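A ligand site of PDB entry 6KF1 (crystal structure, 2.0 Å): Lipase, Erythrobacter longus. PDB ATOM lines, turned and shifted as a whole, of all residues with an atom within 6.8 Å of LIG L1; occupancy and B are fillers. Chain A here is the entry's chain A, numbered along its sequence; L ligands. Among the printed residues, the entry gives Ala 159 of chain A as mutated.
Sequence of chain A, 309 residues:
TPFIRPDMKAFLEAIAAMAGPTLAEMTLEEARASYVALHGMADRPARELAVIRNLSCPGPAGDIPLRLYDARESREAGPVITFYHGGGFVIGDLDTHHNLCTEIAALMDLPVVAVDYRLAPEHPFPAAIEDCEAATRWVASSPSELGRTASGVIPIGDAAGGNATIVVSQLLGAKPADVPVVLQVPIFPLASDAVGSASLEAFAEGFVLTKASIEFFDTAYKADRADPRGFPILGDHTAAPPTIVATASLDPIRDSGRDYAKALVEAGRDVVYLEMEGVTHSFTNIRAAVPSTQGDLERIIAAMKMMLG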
ATOM      1  N   GLY A  87      -5.314 -26.718  15.257  1.00  0.00           N
ATOM      2  CA  GLY A  87      -4.443 -25.981  14.326  1.00  0.00           C
ATOM      3  C   GLY A  87      -4.793 -26.190  12.844  1.00  0.00           C
ATOM      4  O   GLY A  87      -3.852 -26.150  12.006  1.00  0.00           O
ATOM      5  N   GLY A  88      -6.060 -26.401  12.498  1.00  0.00           N
ATOM      6  CA  GLY A  88      -6.522 -26.417  11.099  1.00  0.00           C
ATOM      7  C   GLY A  88      -5.960 -27.539  10.238  1.00  0.00           C
ATOM      8  O   GLY A  88      -6.160 -27.471   9.022  1.00  0.00           O
ATOM      9  N   PHE A  89      -5.388 -28.564  10.879  1.00  0.00           N
ATOM     10  CA  PHE A  89      -4.665 -29.678  10.239  1.00  0.00           C
ATOM     11  C   PHE A  89      -3.397 -29.118   9.573  1.00  0.00           C
ATOM     12  O   PHE A  89      -2.840 -29.837   8.733  1.00  0.00           O
ATOM     13  CB  PHE A  89      -5.541 -30.431   9.243  1.00  0.00           C
ATOM     14  CG  PHE A  89      -6.742 -31.093   9.878  1.00  0.00           C
ATOM     15  CD1 PHE A  89      -6.580 -32.008  10.908  1.00  0.00           C
ATOM     16  CD2 PHE A  89      -8.026 -30.780   9.476  1.00  0.00           C
ATOM     17  CE1 PHE A  89      -7.660 -32.633  11.484  1.00  0.00           C
ATOM     18  CE2 PHE A  89      -9.114 -31.395  10.068  1.00  0.00           C
ATOM     19  CZ  PHE A  89      -8.933 -32.371  11.017  1.00  0.00           C
ATOM     20  N   PHE A 125      -5.697 -33.482   3.170  1.00  0.00           N
ATOM     21  CA  PHE A 125      -6.847 -34.356   3.507  1.00  0.00           C
ATOM     22  C   PHE A 125      -6.799 -35.626   2.656  1.00  0.00           C
ATOM     23  O   PHE A 125      -6.596 -35.527   1.437  1.00  0.00           O
ATOM     24  CB  PHE A 125      -8.124 -33.606   3.190  1.00  0.00           C
ATOM     25  CG  PHE A 125      -9.370 -34.461   3.261  1.00  0.00           C
ATOM     26  CD1 PHE A 125      -9.971 -34.725   4.488  1.00  0.00           C
ATOM     27  CD2 PHE A 125      -9.920 -34.986   2.095  1.00  0.00           C
ATOM     28  CE1 PHE A 125     -11.128 -35.492   4.544  1.00  0.00           C
ATOM     29  CE2 PHE A 125     -11.070 -35.776   2.155  1.00  0.00           C
ATOM     30  CZ  PHE A 125     -11.669 -36.018   3.382  1.00  0.00           C
ATOM     31  N   ALA A 159     -10.985 -28.039  17.990  1.00  0.00           N
ATOM     32  CA  ALA A 159     -10.998 -27.380  16.665  1.00  0.00           C
ATOM     33  C   ALA A 159     -10.827 -28.438  15.569  1.00  0.00           C
ATOM     34  O   ALA A 159     -11.703 -29.348  15.502  1.00  0.00           O
ATOM     35  CB  ALA A 159      -9.928 -26.299  16.674  1.00  0.00           C
ATOM     36  N   ALA A 160      -9.745 -28.424  14.783  1.00  0.00           N
ATOM     37  CA  ALA A 160      -9.475 -29.514  13.810  1.00  0.00           C
ATOM     38  C   ALA A 160      -9.489 -30.865  14.549  1.00  0.00           C
ATOM     39  O   ALA A 160      -9.965 -31.876  13.993  1.00  0.00           O
ATOM     40  CB  ALA A 160      -8.171 -29.310  13.099  1.00  0.00           C
ATOM     41  N   GLY A 161      -9.004 -30.898  15.784  1.00  0.00           N
ATOM     42  CA  GLY A 161      -9.000 -32.106  16.618  1.00  0.00           C
ATOM     43  C   GLY A 161     -10.396 -32.536  17.013  1.00  0.00           C
ATOM     44  O   GLY A 161     -10.595 -33.767  17.204  1.00  0.00           O
ATOM     45  N   GLY A 162     -11.302 -31.582  17.111  1.00  0.00           N
ATOM     46  CA  GLY A 162     -12.738 -31.850  17.367  1.00  0.00           C
ATOM     47  C   GLY A 162     -13.403 -32.444  16.126  1.00  0.00           C
ATOM     48  O   GLY A 162     -14.244 -33.333  16.258  1.00  0.00           O
ATOM     49  N   ASN A 163     -13.040 -31.933  14.949  1.00  0.00           N
ATOM     50  CA  ASN A 163     -13.393 -32.514  13.640  1.00  0.00           C
ATOM     51  C   ASN A 163     -12.907 -33.967  13.627  1.00  0.00           C
ATOM     52  O   ASN A 163     -13.716 -34.880  13.408  1.00  0.00           O
ATOM     53  CB  ASN A 163     -12.779 -31.675  12.512  1.00  0.00           C
ATOM     54  CG  ASN A 163     -12.987 -32.292  11.150  1.00  0.00           C
ATOM     55  OD1 ASN A 163     -12.231 -33.181  10.768  1.00  0.00           O
ATOM     56  ND2 ASN A 163     -13.980 -31.782  10.436  1.00  0.00           N
ATOM     57  N   ALA A 164     -11.624 -34.209  13.924  1.00  0.00           N
ATOM     58  CA  ALA A 164     -11.003 -35.534  13.923  1.00  0.00           C
ATOM     59  C   ALA A 164     -11.709 -36.449  14.918  1.00  0.00           C
ATOM     60  O   ALA A 164     -11.947 -37.642  14.595  1.00  0.00           O
ATOM     61  CB  ALA A 164      -9.520 -35.418  14.186  1.00  0.00           C
ATOM     62  N   PRO A 189     -15.452 -27.950  17.818  1.00  0.00           N
ATOM     63  CA  PRO A 189     -15.201 -28.686  16.606  1.00  0.00           C
ATOM     64  C   PRO A 189     -15.732 -27.992  15.351  1.00  0.00           C
ATOM     65  O   PRO A 189     -16.601 -27.162  15.424  1.00  0.00           O
ATOM     66  CB  PRO A 189     -16.019 -29.962  16.806  1.00  0.00           C
ATOM     67  CG  PRO A 189     -17.211 -29.478  17.590  1.00  0.00           C
ATOM     68  CD  PRO A 189     -16.604 -28.490  18.548  1.00  0.00           C
ATOM     69  N   LEU A 190     -15.103 -28.305  14.228  1.00  0.00           N
ATOM     70  CA  LEU A 190     -15.649 -28.082  12.876  1.00  0.00           C
ATOM     71  C   LEU A 190     -16.406 -29.352  12.508  1.00  0.00           C
ATOM     72  O   LEU A 190     -15.781 -30.377  12.299  1.00  0.00           O
ATOM     73  CB  LEU A 190     -14.518 -27.799  11.900  1.00  0.00           C
ATOM     74  CG  LEU A 190     -14.919 -27.146  10.597  1.00  0.00           C
ATOM     75  CD1 LEU A 190     -15.644 -28.146   9.735  1.00  0.00           C
ATOM     76  CD2 LEU A 190     -15.762 -25.892  10.799  1.00  0.00           C
ATOM     77  N   ALA A 191     -17.722 -29.261  12.432  1.00  0.00           N
ATOM     78  CA  ALA A 191     -18.574 -30.396  12.011  1.00  0.00           C
ATOM     79  C   ALA A 191     -19.267 -30.046  10.712  1.00  0.00           C
ATOM     80  O   ALA A 191     -19.146 -30.810   9.751  1.00  0.00           O
ATOM     81  CB  ALA A 191     -19.555 -30.723  13.119  1.00  0.00           C
ATOM     82  N   ILE A 214      -8.993 -19.506   8.852  1.00  0.00           N
ATOM     83  CA  ILE A 214      -9.875 -20.590   8.334  1.00  0.00           C
ATOM     84  C   ILE A 214      -9.618 -20.762   6.841  1.00  0.00           C
ATOM     85  O   ILE A 214      -9.504 -21.919   6.369  1.00  0.00           O
ATOM     86  CB  ILE A 214     -11.344 -20.274   8.671  1.00  0.00           C
ATOM     87  CG1 ILE A 214     -11.556 -20.420  10.167  1.00  0.00           C
ATOM     88  CG2 ILE A 214     -12.325 -21.098   7.837  1.00  0.00           C
ATOM     89  CD1 ILE A 214     -12.880 -19.918  10.705  1.00  0.00           C
ATOM     90  N   PHE A 217      -6.267 -22.422   6.253  1.00  0.00           N
ATOM     91  CA  PHE A 217      -6.317 -23.866   6.607  1.00  0.00           C
ATOM     92  C   PHE A 217      -7.034 -24.622   5.483  1.00  0.00           C
ATOM     93  O   PHE A 217      -6.605 -25.708   5.063  1.00  0.00           O
ATOM     94  CB  PHE A 217      -7.030 -24.040   7.938  1.00  0.00           C
ATOM     95  CG  PHE A 217      -6.273 -23.478   9.119  1.00  0.00           C
ATOM     96  CD1 PHE A 217      -4.901 -23.601   9.192  1.00  0.00           C
ATOM     97  CD2 PHE A 217      -6.940 -22.913  10.192  1.00  0.00           C
ATOM     98  CE1 PHE A 217      -4.209 -23.129  10.288  1.00  0.00           C
ATOM     99  CE2 PHE A 217      -6.245 -22.487  11.315  1.00  0.00           C
ATOM    100  CZ  PHE A 217      -4.877 -22.559  11.344  1.00  0.00           C
ATOM    101  N   ASP A 218      -8.135 -24.041   5.001  1.00  0.00           N
ATOM    102  CA  ASP A 218      -8.941 -24.708   3.943  1.00  0.00           C
ATOM    103  C   ASP A 218      -8.110 -24.932   2.675  1.00  0.00           C
ATOM    104  O   ASP A 218      -8.157 -26.035   2.110  1.00  0.00           O
ATOM    105  CB  ASP A 218     -10.147 -23.879   3.543  1.00  0.00           C
ATOM    106  CG  ASP A 218     -11.296 -23.999   4.518  1.00  0.00           C
ATOM    107  OD1 ASP A 218     -11.232 -24.896   5.422  1.00  0.00           O
ATOM    108  OD2 ASP A 218     -12.249 -23.210   4.353  1.00  0.00           O
ATOM    109  N   THR A 219      -7.335 -23.921   2.247  1.00  0.00           N
ATOM    110  CA  THR A 219      -6.483 -24.009   1.027  1.00  0.00           C
ATOM    111  C   THR A 219      -5.416 -25.075   1.246  1.00  0.00           C
ATOM    112  O   THR A 219      -5.109 -25.817   0.271  1.00  0.00           O
ATOM    113  CB  THR A 219      -5.873 -22.643   0.702  1.00  0.00           C
ATOM    114  OG1 THR A 219      -6.994 -21.776   0.479  1.00  0.00           O
ATOM    115  CG2 THR A 219      -4.910 -22.667  -0.457  1.00  0.00           C
ATOM    116  N   TYR A 221      -5.439 -27.807   3.433  1.00  0.00           N
ATOM    117  CA  TYR A 221      -5.927 -29.160   3.753  1.00  0.00           C
ATOM    118  C   TYR A 221      -6.707 -29.773   2.563  1.00  0.00           C
ATOM    119  O   TYR A 221      -6.580 -30.978   2.354  1.00  0.00           O
ATOM    120  CB  TYR A 221      -6.764 -29.107   5.039  1.00  0.00           C
ATOM    121  CG  TYR A 221      -7.219 -30.454   5.577  1.00  0.00           C
ATOM    122  CD1 TYR A 221      -6.322 -31.415   6.001  1.00  0.00           C
ATOM    123  CD2 TYR A 221      -8.584 -30.679   5.860  1.00  0.00           C
ATOM    124  CE1 TYR A 221      -6.742 -32.594   6.627  1.00  0.00           C
ATOM    125  CE2 TYR A 221      -8.996 -31.853   6.475  1.00  0.00           C
ATOM    126  CZ  TYR A 221      -8.086 -32.792   6.880  1.00  0.00           C
ATOM    127  OH  TYR A 221      -8.502 -33.954   7.524  1.00  0.00           O
ATOM    128  N   LYS A 222      -7.503 -28.996   1.842  1.00  0.00           N
ATOM    129  CA  LYS A 222      -8.178 -29.458   0.584  1.00  0.00           C
ATOM    130  C   LYS A 222      -9.163 -30.607   0.849  1.00  0.00           C
ATOM    131  O   LYS A 222      -9.172 -31.671   0.130  1.00  0.00           O
ATOM    132  CB  LYS A 222      -7.084 -29.873  -0.395  1.00  0.00           C
ATOM    133  CG  LYS A 222      -6.158 -28.728  -0.779  1.00  0.00           C
ATOM    134  CD  LYS A 222      -5.214 -29.133  -1.896  1.00  0.00           C
ATOM    135  CE  LYS A 222      -4.127 -28.096  -2.157  1.00  0.00           C
ATOM    136  NZ  LYS A 222      -4.709 -26.752  -2.451  1.00  0.00           N
ATOM    137  N   ALA A 223     -10.003 -30.443   1.867  1.00  0.00           N
ATOM    138  CA  ALA A 223     -11.055 -31.397   2.202  1.00  0.00           C
ATOM    139  C   ALA A 223     -12.208 -31.149   1.221  1.00  0.00           C
ATOM    140  O   ALA A 223     -12.663 -30.055   1.177  1.00  0.00           O
ATOM    141  CB  ALA A 223     -11.516 -31.191   3.629  1.00  0.00           C
ATOM    142  N   ASP A 224     -12.759 -32.171   0.631  1.00  0.00           N
ATOM    143  CA  ASP A 224     -13.949 -32.042  -0.251  1.00  0.00           C
ATOM    144  C   ASP A 224     -15.172 -31.734   0.630  1.00  0.00           C
ATOM    145  O   ASP A 224     -15.471 -32.478   1.582  1.00  0.00           O
ATOM    146  CB  ASP A 224     -14.163 -33.314  -1.076  1.00  0.00           C
ATOM    147  CG  ASP A 224     -15.222 -33.062  -2.135  1.00  0.00           C
ATOM    148  OD1 ASP A 224     -16.360 -32.973  -1.745  1.00  0.00           O
ATOM    149  OD2 ASP A 224     -14.852 -32.764  -3.303  1.00  0.00           O
ATOM    150  N   ARG A 225     -15.900 -30.659   0.297  1.00  0.00           N
ATOM    151  CA  ARG A 225     -17.085 -30.206   1.064  1.00  0.00           C
ATOM    152  C   ARG A 225     -18.170 -31.262   1.045  1.00  0.00           C
ATOM    153  O   ARG A 225     -19.092 -31.143   1.879  1.00  0.00           O
ATOM    154  CB  ARG A 225     -17.671 -28.867   0.580  1.00  0.00           C
ATOM    155  CG  ARG A 225     -16.788 -27.633   0.732  1.00  0.00           C
ATOM    156  CD  ARG A 225     -16.250 -27.344   2.091  1.00  0.00           C
ATOM    157  NE  ARG A 225     -15.620 -26.037   2.269  1.00  0.00           N
ATOM    158  CZ  ARG A 225     -14.301 -25.814   2.433  1.00  0.00           C
ATOM    159  NH1 ARG A 225     -13.406 -26.784   2.428  1.00  0.00           N
ATOM    160  NH2 ARG A 225     -13.878 -24.579   2.591  1.00  0.00           N
ATOM    161  N   GLY A 230     -14.382 -34.937   5.905  1.00  0.00           N
ATOM    162  CA  GLY A 230     -14.038 -33.515   6.014  1.00  0.00           C
ATOM    163  C   GLY A 230     -15.084 -32.741   6.801  1.00  0.00           C
ATOM    164  O   GLY A 230     -14.726 -31.866   7.626  1.00  0.00           O
ATOM    165  N   PHE A 231     -16.368 -33.054   6.580  1.00  0.00           N
ATOM    166  CA  PHE A 231     -17.490 -32.326   7.212  1.00  0.00           C
ATOM    167  C   PHE A 231     -18.421 -33.364   7.838  1.00  0.00           C
ATOM    168  O   PHE A 231     -19.429 -33.763   7.204  1.00  0.00           O
ATOM    169  CB  PHE A 231     -18.143 -31.382   6.205  1.00  0.00           C
ATOM    170  CG  PHE A 231     -17.140 -30.402   5.664  1.00  0.00           C
ATOM    171  CD1 PHE A 231     -16.259 -30.781   4.677  1.00  0.00           C
ATOM    172  CD2 PHE A 231     -16.991 -29.159   6.241  1.00  0.00           C
ATOM    173  CE1 PHE A 231     -15.284 -29.893   4.224  1.00  0.00           C
ATOM    174  CE2 PHE A 231     -16.024 -28.270   5.784  1.00  0.00           C
ATOM    175  CZ  PHE A 231     -15.138 -28.659   4.805  1.00  0.00           C
ATOM    176  N   ILE A 253     -16.523 -20.465  14.510  1.00  0.00           N
ATOM    177  CA  ILE A 253     -17.087 -21.797  14.179  1.00  0.00           C
ATOM    178  C   ILE A 253     -18.040 -22.316  15.284  1.00  0.00           C
ATOM    179  O   ILE A 253     -18.428 -23.554  15.262  1.00  0.00           O
ATOM    180  CB  ILE A 253     -15.987 -22.779  13.832  1.00  0.00           C
ATOM    181  CG1 ILE A 253     -15.161 -23.224  15.030  1.00  0.00           C
ATOM    182  CG2 ILE A 253     -15.140 -22.201  12.700  1.00  0.00           C
ATOM    183  CD1 ILE A 253     -14.349 -24.482  14.762  1.00  0.00           C
HETATM  184  C1  LIG L   1     -10.866 -28.285   8.894  1.00  0.00           C
HETATM  185  C2  LIG L   1     -12.010 -28.903   8.389  1.00  0.00           C
HETATM  186  C3  LIG L   1     -12.220 -28.877   7.026  1.00  0.00           C
HETATM  187  C4  LIG L   1     -11.336 -28.217   6.197  1.00  0.00           C
HETATM  188  C5  LIG L   1     -10.202 -27.612   6.718  1.00  0.00           C
HETATM  189  C6  LIG L   1      -9.948 -27.636   8.065  1.00  0.00           C
HETATM  190  O1  LIG L   1     -11.572 -28.208   4.856  1.00  0.00           O
HETATM  191  N1  LIG L   1     -10.666 -28.299  10.334  1.00  0.00           N
HETATM  192  O2  LIG L   1      -9.748 -27.621  10.797  1.00  0.00           O
HETATM  193  O3  LIG L   1     -11.470 -28.933  11.013  1.00  0.00           O
HETATM  194  C1  LG2 L   2     -10.946 -24.556  10.916  1.00  0.00           C
HETATM  195  C2  LG2 L   2     -12.325 -24.375  10.845  1.00  0.00           C
HETATM  196  C3  LG2 L   2     -12.939 -24.353   9.610  1.00  0.00           C
HETATM  197  C4  LG2 L   2     -12.210 -24.510   8.426  1.00  0.00           C
HETATM  198  C5  LG2 L   2     -10.819 -24.689   8.516  1.00  0.00           C
HETATM  199  C6  LG2 L   2     -10.191 -24.716   9.748  1.00  0.00           C
HETATM  200  O1  LG2 L   2     -12.904 -24.506   7.222  1.00  0.00           O
HETATM  201  N1  LG2 L   2     -10.326 -24.640  12.228  1.00  0.00           N
HETATM  202  O2  LG2 L   2      -9.135 -24.515  12.316  1.00  0.00           O
HETATM  203  O3  LG2 L   2     -11.039 -24.875  13.199  1.00  0.00           O
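An oxygen (O1) of LIG L1 lies close to the side-chain carboxylate (OD1) of Asp 218 (3.4 Å).
The guanidinium group (NH1) of Arg 225 lies within hydrogen-bond range of an oxygen (O1) of LIG L1 (3.4 Å).
An oxygen (O1) of LG2 L2 is in hydrogen-bond range of the side-chain carboxylate (OD1) of Asp 218 (2.5 Å).
The side-chain carboxylate of Asp 218 is in salt-bridge range of the guanidinium group of Arg 225, at 2.8 Å.
O of Leu 190 sits at hydrogen-bond distance from ND2 of Asn 163 (2.9 Å).
O of Gly 230 sits at hydrogen-bond distance from ND2 of Asn 163.
The backbone carbonyl oxygen (O) of Tyr 221 sits at hydrogen-bond distance from the backbone NH (N) of Phe 125.
Merely in contact with LIG L1: Ala 223, Ala 160, Leu 190, Asn 163, Gly 88, Phe 89, Tyr 221, Phe 231 and Gly 230.
Hydrophobic or aromatic side chains that line LIG L1: Phe 89, Ala 160, Leu 190, Tyr 221, Ala 223 and Phe 231.
11 residues have an atom within 4 Å of LIG L1: Gly 88, Phe 89, Ala 160, Asn 163, Leu 190, Asp 218, Tyr 221, Ala 223, Arg 225, Gly 230 and Phe 231.
The nearest printed residue that does not touch LIG L1 is Phe 217 (4.4 Å).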
